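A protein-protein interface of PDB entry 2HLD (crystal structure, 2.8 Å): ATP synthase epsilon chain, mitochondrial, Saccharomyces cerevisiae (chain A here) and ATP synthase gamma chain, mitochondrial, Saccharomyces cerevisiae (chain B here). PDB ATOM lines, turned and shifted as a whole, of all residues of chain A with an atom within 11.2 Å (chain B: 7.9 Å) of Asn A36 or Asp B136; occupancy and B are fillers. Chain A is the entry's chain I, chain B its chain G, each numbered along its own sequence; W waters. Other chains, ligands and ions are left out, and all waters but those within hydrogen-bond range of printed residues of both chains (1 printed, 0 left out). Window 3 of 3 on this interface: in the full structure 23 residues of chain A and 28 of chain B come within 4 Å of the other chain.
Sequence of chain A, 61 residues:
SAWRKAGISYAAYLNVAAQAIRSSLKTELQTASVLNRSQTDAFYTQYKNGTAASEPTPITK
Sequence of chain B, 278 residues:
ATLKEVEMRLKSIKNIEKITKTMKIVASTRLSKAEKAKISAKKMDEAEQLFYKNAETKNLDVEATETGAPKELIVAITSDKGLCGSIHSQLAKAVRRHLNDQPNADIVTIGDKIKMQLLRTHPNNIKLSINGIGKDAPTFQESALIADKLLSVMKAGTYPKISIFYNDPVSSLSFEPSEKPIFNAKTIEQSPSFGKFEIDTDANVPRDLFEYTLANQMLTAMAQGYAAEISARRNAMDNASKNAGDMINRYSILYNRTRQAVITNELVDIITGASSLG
Asn A36 touches one residue of chain B. No residue of chain B comes within 4 Å of Leu A35. Of chain B, only Gln B141 comes within 4 Å of Gln A39. No residue of chain A comes within 4 Å of Gly B134. Of chain A, only Asp A41 (3.6 Å) comes within 4 Å of Lys B135. No residue of chain A comes within 4 Å of Ala B137. No residue of chain A comes within 4 Å of Pro B138. Printed residues of chain B within 4 Å of Ser A38: Gln B141 (3.3 Å). Printed residues of chain A within 4 Å of Lys B33: Ser A33 (3.5 Å). Ala A32 touches none of the printed residues of chain B. The nearest residue of chain B that does not touch Asn A36 is Thr B139 (4.7 Å).
The side-chain amino group of Lys B135 is in salt-bridge range of the side-chain carboxylate of Asp A41 (3.6 Å). The side-chain amide oxygen (OE1) of Gln B141 sits close to the backbone carbonyl oxygen (O) of Ser A38 (3.5 Å). The backbone NH of Gln A39 lies within hydrogen-bond range of the side-chain amide oxygen of Gln B141.
Water W1 bridges N of Gln B141 (3.2 Å) and O of Arg A37 (3.4 Å).
Hydrophobic or aromatic side chains of chain B within 4 Å of the printed part of chain A: Ile B133. Of the 19 printed residues of chain A, 9 touch a printed residue of chain B. Among the printed residues, 12 pairs touch across the chains.
OH of Tyr B226 is in hydrogen-bond range of O of Lys B135 (3.3 Å).
CG of Gln B141 touches ND2 of Asn A15, at 3.3 Å. Lys B33 touches Ser A33. Asn A36 touches Asp B136. O of Arg A37 touches CB of Gln B141, at 3.8 Å. OE1 of Gln B141 touches N of Thr A40, at 3.9 Å. CB of Thr A40 touches OE2 of Glu B142, at 3.4 Å. O of Asp A41 touches O of Gly B132, at 3.96 Å. Gly B132 touches Ala A42 (O to CA, 3.98 Å). Ile B133 touches Ala A42.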
ATOM      1  N   ASN A  15     -20.998  20.541  -3.052  1.00  0.00           N
ATOM      2  CA  ASN A  15     -19.543  20.487  -3.202  1.00  0.00           C
ATOM      3  C   ASN A  15     -19.068  21.395  -4.336  1.00  0.00           C
ATOM      4  O   ASN A  15     -18.172  22.231  -4.149  1.00  0.00           O
ATOM      5  CB  ASN A  15     -19.084  19.043  -3.452  1.00  0.00           C
ATOM      6  CG  ASN A  15     -17.626  18.948  -3.922  1.00  0.00           C
ATOM      7  OD1 ASN A  15     -17.349  18.531  -5.052  1.00  0.00           O
ATOM      8  ND2 ASN A  15     -16.695  19.333  -3.055  1.00  0.00           N
ATOM      9  N   ALA A  18     -19.279  24.894  -3.629  1.00  0.00           N
ATOM     10  CA  ALA A  18     -18.276  25.281  -2.640  1.00  0.00           C
ATOM     11  C   ALA A  18     -16.889  25.297  -3.272  1.00  0.00           C
ATOM     12  O   ALA A  18     -15.964  25.909  -2.723  1.00  0.00           O
ATOM     13  CB  ALA A  18     -18.312  24.337  -1.430  1.00  0.00           C
ATOM     14  N   GLN A  19     -16.753  24.619  -4.416  1.00  0.00           N
ATOM     15  CA  GLN A  19     -15.475  24.549  -5.131  1.00  0.00           C
ATOM     16  C   GLN A  19     -15.347  25.633  -6.186  1.00  0.00           C
ATOM     17  O   GLN A  19     -14.231  25.983  -6.585  1.00  0.00           O
ATOM     18  CB  GLN A  19     -15.241  23.182  -5.785  1.00  0.00           C
ATOM     19  CG  GLN A  19     -13.747  22.834  -5.908  1.00  0.00           C
ATOM     20  CD  GLN A  19     -13.379  22.150  -7.218  1.00  0.00           C
ATOM     21  OE1 GLN A  19     -14.252  21.718  -7.973  1.00  0.00           O
ATOM     22  NE2 GLN A  19     -12.080  22.054  -7.489  1.00  0.00           N
ATOM     23  N   ARG A  22     -14.586  28.584  -4.337  1.00  0.00           N
ATOM     24  CA  ARG A  22     -13.176  28.474  -4.013  1.00  0.00           C
ATOM     25  C   ARG A  22     -12.415  29.112  -5.174  1.00  0.00           C
ATOM     26  O   ARG A  22     -12.044  30.286  -5.093  1.00  0.00           O
ATOM     27  CB  ARG A  22     -12.767  27.016  -3.780  1.00  0.00           C
ATOM     28  N   SER A  23     -12.232  28.356  -6.262  1.00  0.00           N
ATOM     29  CA  SER A  23     -11.539  28.839  -7.465  1.00  0.00           C
ATOM     30  C   SER A  23     -12.127  30.155  -8.022  1.00  0.00           C
ATOM     31  O   SER A  23     -11.628  31.258  -7.745  1.00  0.00           O
ATOM     32  CB  SER A  23     -11.533  27.751  -8.547  1.00  0.00           C
ATOM     33  N   LEU A  29      -5.969  35.208  -0.307  1.00  0.00           N
ATOM     34  CA  LEU A  29      -6.927  34.647   0.644  1.00  0.00           C
ATOM     35  C   LEU A  29      -7.087  33.145   0.387  1.00  0.00           C
ATOM     36  O   LEU A  29      -7.692  32.428   1.194  1.00  0.00           O
ATOM     37  CB  LEU A  29      -8.282  35.356   0.529  1.00  0.00           C
ATOM     38  CG  LEU A  29      -8.374  36.806   1.035  1.00  0.00           C
ATOM     39  CD1 LEU A  29      -9.567  37.534   0.402  1.00  0.00           C
ATOM     40  CD2 LEU A  29      -8.417  36.901   2.573  1.00  0.00           C
ATOM     41  N   GLN A  30      -6.524  32.687  -0.735  1.00  0.00           N
ATOM     42  CA  GLN A  30      -6.575  31.293  -1.154  1.00  0.00           C
ATOM     43  C   GLN A  30      -5.359  30.504  -0.683  1.00  0.00           C
ATOM     44  O   GLN A  30      -4.592  29.990  -1.505  1.00  0.00           O
ATOM     45  CB  GLN A  30      -6.692  31.211  -2.676  1.00  0.00           C
ATOM     46  CG  GLN A  30      -8.083  31.529  -3.220  1.00  0.00           C
ATOM     47  CD  GLN A  30      -8.257  31.141  -4.689  1.00  0.00           C
ATOM     48  OE1 GLN A  30      -7.319  30.636  -5.336  1.00  0.00           O
ATOM     49  NE2 GLN A  30      -9.459  31.379  -5.219  1.00  0.00           N
ATOM     50  N   THR A  31      -5.210  30.401   0.637  1.00  0.00           N
ATOM     51  CA  THR A  31      -4.096  29.698   1.294  1.00  0.00           C
ATOM     52  C   THR A  31      -3.890  28.236   0.817  1.00  0.00           C
ATOM     53  O   THR A  31      -4.495  27.809  -0.167  1.00  0.00           O
ATOM     54  CB  THR A  31      -4.223  29.842   2.856  1.00  0.00           C
ATOM     55  OG1 THR A  31      -3.447  28.840   3.536  1.00  0.00           O
ATOM     56  CG2 THR A  31      -5.648  29.574   3.326  1.00  0.00           C
ATOM     57  N   ALA A  32      -3.007  27.488   1.485  1.00  0.00           N
ATOM     58  CA  ALA A  32      -2.675  26.111   1.082  1.00  0.00           C
ATOM     59  C   ALA A  32      -3.803  25.119   1.381  1.00  0.00           C
ATOM     60  O   ALA A  32      -4.179  24.315   0.519  1.00  0.00           O
ATOM     61  CB  ALA A  32      -1.372  25.656   1.742  1.00  0.00           C
ATOM     62  N   SER A  33      -4.340  25.196   2.601  1.00  0.00           N
ATOM     63  CA  SER A  33      -5.432  24.327   3.060  1.00  0.00           C
ATOM     64  C   SER A  33      -6.776  24.597   2.354  1.00  0.00           C
ATOM     65  O   SER A  33      -7.768  23.899   2.612  1.00  0.00           O
ATOM     66  CB  SER A  33      -5.596  24.437   4.580  1.00  0.00           C
ATOM     67  OG  SER A  33      -5.855  25.776   4.955  1.00  0.00           O
ATOM     68  N   VAL A  34      -6.796  25.617   1.490  1.00  0.00           N
ATOM     69  CA  VAL A  34      -7.925  25.898   0.596  1.00  0.00           C
ATOM     70  C   VAL A  34      -7.703  25.156  -0.722  1.00  0.00           C
ATOM     71  O   VAL A  34      -8.571  24.419  -1.182  1.00  0.00           O
ATOM     72  CB  VAL A  34      -8.135  27.441   0.369  1.00  0.00           C
ATOM     73  CG1 VAL A  34      -8.995  27.734  -0.871  1.00  0.00           C
ATOM     74  CG2 VAL A  34      -8.736  28.105   1.616  1.00  0.00           C
ATOM     75  N   LEU A  35      -6.531  25.333  -1.319  1.00  0.00           N
ATOM     76  CA  LEU A  35      -6.195  24.610  -2.542  1.00  0.00           C
ATOM     77  C   LEU A  35      -6.208  23.089  -2.315  1.00  0.00           C
ATOM     78  O   LEU A  35      -6.410  22.324  -3.261  1.00  0.00           O
ATOM     79  CB  LEU A  35      -4.841  25.078  -3.099  1.00  0.00           C
ATOM     80  N   ASN A  36      -6.008  22.675  -1.059  1.00  0.00           N
ATOM     81  CA  ASN A  36      -5.963  21.253  -0.665  1.00  0.00           C
ATOM     82  C   ASN A  36      -7.352  20.641  -0.447  1.00  0.00           C
ATOM     83  O   ASN A  36      -7.624  19.520  -0.871  1.00  0.00           O
ATOM     84  CB  ASN A  36      -5.082  21.057   0.588  1.00  0.00           C
ATOM     85  CG  ASN A  36      -3.580  20.866   0.254  1.00  0.00           C
ATOM     86  OD1 ASN A  36      -3.147  20.963  -0.905  1.00  0.00           O
ATOM     87  ND2 ASN A  36      -2.789  20.590   1.285  1.00  0.00           N
ATOM     88  N   ARG A  37      -8.211  21.403   0.224  1.00  0.00           N
ATOM     89  CA  ARG A  37      -9.622  21.096   0.405  1.00  0.00           C
ATOM     90  C   ARG A  37     -10.339  20.933  -0.943  1.00  0.00           C
ATOM     91  O   ARG A  37     -11.472  20.437  -1.002  1.00  0.00           O
ATOM     92  CB  ARG A  37     -10.254  22.200   1.258  1.00  0.00           C
ATOM     93  CG  ARG A  37     -11.701  22.554   0.957  1.00  0.00           C
ATOM     94  CD  ARG A  37     -12.173  23.840   1.609  1.00  0.00           C
ATOM     95  NE  ARG A  37     -11.620  24.007   2.954  1.00  0.00           N
ATOM     96  CZ  ARG A  37     -11.510  25.170   3.596  1.00  0.00           C
ATOM     97  NH1 ARG A  37     -11.926  26.303   3.039  1.00  0.00           N
ATOM     98  NH2 ARG A  37     -10.978  25.200   4.809  1.00  0.00           N
ATOM     99  N   SER A  38      -9.666  21.329  -2.023  1.00  0.00           N
ATOM    100  CA  SER A  38     -10.194  21.148  -3.375  1.00  0.00           C
ATOM    101  C   SER A  38      -9.463  20.017  -4.127  1.00  0.00           C
ATOM    102  O   SER A  38      -9.640  19.862  -5.336  1.00  0.00           O
ATOM    103  CB  SER A  38     -10.149  22.474  -4.169  1.00  0.00           C
ATOM    104  OG  SER A  38     -11.229  23.361  -3.857  1.00  0.00           O
ATOM    105  N   GLN A  39      -8.657  19.224  -3.412  1.00  0.00           N
ATOM    106  CA  GLN A  39      -7.846  18.149  -4.035  1.00  0.00           C
ATOM    107  C   GLN A  39      -7.941  16.774  -3.338  1.00  0.00           C
ATOM    108  O   GLN A  39      -7.742  16.664  -2.122  1.00  0.00           O
ATOM    109  CB  GLN A  39      -6.370  18.581  -4.152  1.00  0.00           C
ATOM    110  N   THR A  40      -8.226  15.734  -4.122  1.00  0.00           N
ATOM    111  CA  THR A  40      -8.347  14.362  -3.604  1.00  0.00           C
ATOM    112  C   THR A  40      -7.656  13.354  -4.519  1.00  0.00           C
ATOM    113  O   THR A  40      -7.861  13.362  -5.739  1.00  0.00           O
ATOM    114  CB  THR A  40      -9.833  13.961  -3.429  1.00  0.00           C
ATOM    115  N   ASP A  41      -6.850  12.480  -3.921  1.00  0.00           N
ATOM    116  CA  ASP A  41      -6.151  11.444  -4.672  1.00  0.00           C
ATOM    117  C   ASP A  41      -6.843  10.109  -4.469  1.00  0.00           C
ATOM    118  O   ASP A  41      -6.225   9.051  -4.580  1.00  0.00           O
ATOM    119  CB  ASP A  41      -4.688  11.360  -4.223  1.00  0.00           C
ATOM    120  CG  ASP A  41      -3.975  12.703  -4.299  1.00  0.00           C
ATOM    121  OD1 ASP A  41      -4.034  13.352  -5.374  1.00  0.00           O
ATOM    122  OD2 ASP A  41      -3.336  13.184  -3.333  1.00  0.00           O
ATOM    123  N   ALA A  42      -8.137  10.174  -4.186  1.00  0.00           N
ATOM    124  CA  ALA A  42      -8.896   9.002  -3.785  1.00  0.00           C
ATOM    125  C   ALA A  42      -9.491   8.223  -4.964  1.00  0.00           C
ATOM    126  O   ALA A  42      -9.868   8.808  -5.976  1.00  0.00           O
ATOM    127  CB  ALA A  42      -9.971   9.404  -2.798  1.00  0.00           C
ATOM    128  N   ARG B  30       1.230  16.970  12.809  1.00  0.00           N
ATOM    129  CA  ARG B  30       0.125  16.481  11.984  1.00  0.00           C
ATOM    130  C   ARG B  30      -1.147  16.332  12.808  1.00  0.00           C
ATOM    131  O   ARG B  30      -2.254  16.436  12.267  1.00  0.00           O
ATOM    132  CB  ARG B  30       0.496  15.136  11.360  1.00  0.00           C
ATOM    133  CG  ARG B  30      -0.098  14.903  10.002  1.00  0.00           C
ATOM    134  CD  ARG B  30       0.321  13.601   9.355  1.00  0.00           C
ATOM    135  NE  ARG B  30       1.604  13.719   8.668  1.00  0.00           N
ATOM    136  CZ  ARG B  30       2.020  12.901   7.705  1.00  0.00           C
ATOM    137  NH1 ARG B  30       1.248  11.894   7.303  1.00  0.00           N
ATOM    138  NH2 ARG B  30       3.205  13.090   7.134  1.00  0.00           N
ATOM    139  N   LYS B  33      -2.789  19.913  13.616  1.00  0.00           N
ATOM    140  CA  LYS B  33      -3.535  20.277  12.415  1.00  0.00           C
ATOM    141  C   LYS B  33      -4.836  19.441  12.319  1.00  0.00           C
ATOM    142  O   LYS B  33      -5.792  19.831  11.640  1.00  0.00           O
ATOM    143  CB  LYS B  33      -2.627  20.110  11.183  1.00  0.00           C
ATOM    144  CG  LYS B  33      -3.255  20.393   9.811  1.00  0.00           C
ATOM    145  CD  LYS B  33      -3.259  21.877   9.427  1.00  0.00           C
ATOM    146  CE  LYS B  33      -4.070  22.100   8.140  1.00  0.00           C
ATOM    147  NZ  LYS B  33      -4.132  23.521   7.678  1.00  0.00           N
ATOM    148  N   LYS B  81      -2.624   3.384   5.590  1.00  0.00           N
ATOM    149  CA  LYS B  81      -1.340   3.404   6.275  1.00  0.00           C
ATOM    150  C   LYS B  81      -1.328   2.549   7.528  1.00  0.00           C
ATOM    151  O   LYS B  81      -2.271   2.580   8.318  1.00  0.00           O
ATOM    152  CB  LYS B  81      -0.987   4.836   6.661  1.00  0.00           C
ATOM    153  CG  LYS B  81      -0.831   5.791   5.503  1.00  0.00           C
ATOM    154  CD  LYS B  81      -0.717   7.210   6.028  1.00  0.00           C
ATOM    155  CE  LYS B  81      -0.103   8.155   4.994  1.00  0.00           C
ATOM    156  NZ  LYS B  81       1.394   8.148   5.013  1.00  0.00           N
ATOM    157  N   GLY B 132      -6.666   5.233  -1.020  1.00  0.00           N
ATOM    158  CA  GLY B 132      -5.756   6.373  -0.980  1.00  0.00           C
ATOM    159  C   GLY B 132      -6.277   7.520  -0.146  1.00  0.00           C
ATOM    160  O   GLY B 132      -6.471   8.631  -0.652  1.00  0.00           O
ATOM    161  N   ILE B 133      -6.497   7.237   1.135  1.00  0.00           N
ATOM    162  CA  ILE B 133      -7.074   8.189   2.068  1.00  0.00           C
ATOM    163  C   ILE B 133      -6.044   8.599   3.110  1.00  0.00           C
ATOM    164  O   ILE B 133      -6.059   9.735   3.604  1.00  0.00           O
ATOM    165  CB  ILE B 133      -8.334   7.566   2.741  1.00  0.00           C
ATOM    166  CG1 ILE B 133      -9.472   7.418   1.719  1.00  0.00           C
ATOM    167  CG2 ILE B 133      -8.800   8.390   3.960  1.00  0.00           C
ATOM    168  CD1 ILE B 133      -9.863   8.720   0.990  1.00  0.00           C
ATOM    169  N   GLY B 134      -5.143   7.670   3.427  1.00  0.00           N
ATOM    170  CA  GLY B 134      -4.121   7.866   4.461  1.00  0.00           C
ATOM    171  C   GLY B 134      -3.517   9.258   4.639  1.00  0.00           C
ATOM    172  O   GLY B 134      -3.557   9.807   5.741  1.00  0.00           O
ATOM    173  N   LYS B 135      -2.985   9.823   3.549  1.00  0.00           N
ATOM    174  CA  LYS B 135      -2.072  10.989   3.578  1.00  0.00           C
ATOM    175  C   LYS B 135      -2.567  12.262   4.280  1.00  0.00           C
ATOM    176  O   LYS B 135      -2.283  12.480   5.464  1.00  0.00           O
ATOM    177  CB  LYS B 135      -1.616  11.338   2.151  1.00  0.00           C
ATOM    178  CG  LYS B 135      -0.446  10.504   1.611  1.00  0.00           C
ATOM    179  CD  LYS B 135      -0.212  10.766   0.111  1.00  0.00           C
ATOM    180  CE  LYS B 135      -1.213   9.990  -0.767  1.00  0.00           C
ATOM    181  NZ  LYS B 135      -1.245  10.460  -2.185  1.00  0.00           N
ATOM    182  N   ASP B 136      -3.276  13.108   3.530  1.00  0.00           N
ATOM    183  CA  ASP B 136      -3.743  14.410   4.021  1.00  0.00           C
ATOM    184  C   ASP B 136      -4.941  14.263   4.968  1.00  0.00           C
ATOM    185  O   ASP B 136      -5.483  13.172   5.118  1.00  0.00           O
ATOM    186  CB  ASP B 136      -4.109  15.326   2.837  1.00  0.00           C
ATOM    187  CG  ASP B 136      -2.896  16.071   2.251  1.00  0.00           C
ATOM    188  OD1 ASP B 136      -2.129  15.459   1.477  1.00  0.00           O
ATOM    189  OD2 ASP B 136      -2.651  17.282   2.483  1.00  0.00           O
ATOM    190  N   ALA B 137      -5.346  15.367   5.599  1.00  0.00           N
ATOM    191  CA  ALA B 137      -6.570  15.427   6.412  1.00  0.00           C
ATOM    192  C   ALA B 137      -7.814  15.125   5.570  1.00  0.00           C
ATOM    193  O   ALA B 137      -7.766  15.258   4.351  1.00  0.00           O
ATOM    194  CB  ALA B 137      -6.693  16.784   7.076  1.00  0.00           C
ATOM    195  N   PRO B 138      -8.912  14.689   6.192  1.00  0.00           N
ATOM    196  CA  PRO B 138     -10.151  14.454   5.446  1.00  0.00           C
ATOM    197  C   PRO B 138     -10.897  15.756   5.114  1.00  0.00           C
ATOM    198  O   PRO B 138     -10.853  16.727   5.888  1.00  0.00           O
ATOM    199  CB  PRO B 138     -10.964  13.575   6.395  1.00  0.00           C
ATOM    200  CG  PRO B 138     -10.500  13.961   7.745  1.00  0.00           C
ATOM    201  CD  PRO B 138      -9.063  14.367   7.625  1.00  0.00           C
ATOM    202  N   THR B 139     -11.566  15.760   3.963  1.00  0.00           N
ATOM    203  CA  THR B 139     -12.251  16.951   3.451  1.00  0.00           C
ATOM    204  C   THR B 139     -13.653  16.650   2.885  1.00  0.00           C
ATOM    205  O   THR B 139     -13.863  15.604   2.266  1.00  0.00           O
ATOM    206  CB  THR B 139     -11.409  17.589   2.337  1.00  0.00           C
ATOM    207  OG1 THR B 139     -11.198  16.621   1.300  1.00  0.00           O
ATOM    208  CG2 THR B 139     -10.003  17.921   2.828  1.00  0.00           C
ATOM    209  N   GLN B 141     -14.991  17.418   0.279  1.00  0.00           N
ATOM    210  CA  GLN B 141     -15.005  17.023  -1.126  1.00  0.00           C
ATOM    211  C   GLN B 141     -14.929  15.501  -1.298  1.00  0.00           C
ATOM    212  O   GLN B 141     -15.532  14.942  -2.221  1.00  0.00           O
ATOM    213  CB  GLN B 141     -13.891  17.715  -1.919  1.00  0.00           C
ATOM    214  CG  GLN B 141     -14.017  17.493  -3.416  1.00  0.00           C
ATOM    215  CD  GLN B 141     -12.725  17.700  -4.163  1.00  0.00           C
ATOM    216  OE1 GLN B 141     -11.639  17.605  -3.584  1.00  0.00           O
ATOM    217  NE2 GLN B 141     -12.834  17.980  -5.460  1.00  0.00           N
ATOM    218  N   GLU B 142     -14.186  14.842  -0.412  1.00  0.00           N
ATOM    219  CA  GLU B 142     -14.048  13.386  -0.470  1.00  0.00           C
ATOM    220  C   GLU B 142     -15.287  12.723   0.110  1.00  0.00           C
ATOM    221  O   GLU B 142     -15.885  11.839  -0.506  1.00  0.00           O
ATOM    222  CB  GLU B 142     -12.801  12.936   0.286  1.00  0.00           C
ATOM    223  CG  GLU B 142     -11.545  13.659  -0.160  1.00  0.00           C
ATOM    224  CD  GLU B 142     -10.291  13.103   0.469  1.00  0.00           C
ATOM    225  OE1 GLU B 142     -10.173  13.179   1.718  1.00  0.00           O
ATOM    226  OE2 GLU B 142      -9.423  12.613  -0.300  1.00  0.00           O
ATOM    227  N   TYR B 226      -9.129   9.847  11.651  1.00  0.00           N
ATOM    228  CA  TYR B 226      -7.852  10.500  11.366  1.00  0.00           C
ATOM    229  C   TYR B 226      -7.161  10.889  12.661  1.00  0.00           C
ATOM    230  O   TYR B 226      -6.106  10.361  12.986  1.00  0.00           O
ATOM    231  CB  TYR B 226      -8.096  11.752  10.535  1.00  0.00           C
ATOM    232  CG  TYR B 226      -6.884  12.371   9.881  1.00  0.00           C
ATOM    233  CD1 TYR B 226      -6.374  11.852   8.687  1.00  0.00           C
ATOM    234  CD2 TYR B 226      -6.273  13.510  10.420  1.00  0.00           C
ATOM    235  CE1 TYR B 226      -5.270  12.429   8.054  1.00  0.00           C
ATOM    236  CE2 TYR B 226      -5.163  14.103   9.796  1.00  0.00           C
ATOM    237  CZ  TYR B 226      -4.665  13.555   8.608  1.00  0.00           C
ATOM    238  OH  TYR B 226      -3.574  14.117   7.961  1.00  0.00           O
ATOM    239  N   GLU B 229      -6.021   7.996  14.501  1.00  0.00           N
ATOM    240  CA  GLU B 229      -4.939   7.291  13.834  1.00  0.00           C
ATOM    241  C   GLU B 229      -3.614   8.011  14.086  1.00  0.00           C
ATOM    242  O   GLU B 229      -2.648   7.400  14.538  1.00  0.00           O
ATOM    243  CB  GLU B 229      -5.224   7.203  12.339  1.00  0.00           C
ATOM    244  CG  GLU B 229      -4.522   6.079  11.600  1.00  0.00           C
ATOM    245  CD  GLU B 229      -4.586   6.244  10.081  1.00  0.00           C
ATOM    246  OE1 GLU B 229      -5.464   6.988   9.586  1.00  0.00           O
ATOM    247  OE2 GLU B 229      -3.756   5.639   9.363  1.00  0.00           O
ATOM    248  N   ILE B 230      -3.589   9.313  13.807  1.00  0.00           N
ATOM    249  CA  ILE B 230      -2.415  10.145  14.022  1.00  0.00           C
ATOM    250  C   ILE B 230      -1.932  10.072  15.471  1.00  0.00           C
ATOM    251  O   ILE B 230      -0.735   9.991  15.715  1.00  0.00           O
ATOM    252  CB  ILE B 230      -2.682  11.599  13.568  1.00  0.00           C
ATOM    253  CG1 ILE B 230      -3.052  11.650  12.079  1.00  0.00           C
ATOM    254  CG2 ILE B 230      -1.476  12.485  13.819  1.00  0.00           C
ATOM    255  CD1 ILE B 230      -2.019  11.029  11.124  1.00  0.00           C
HETATM  256  O   HOH W   1     -13.600  19.950   1.583  1.00  0.00           O
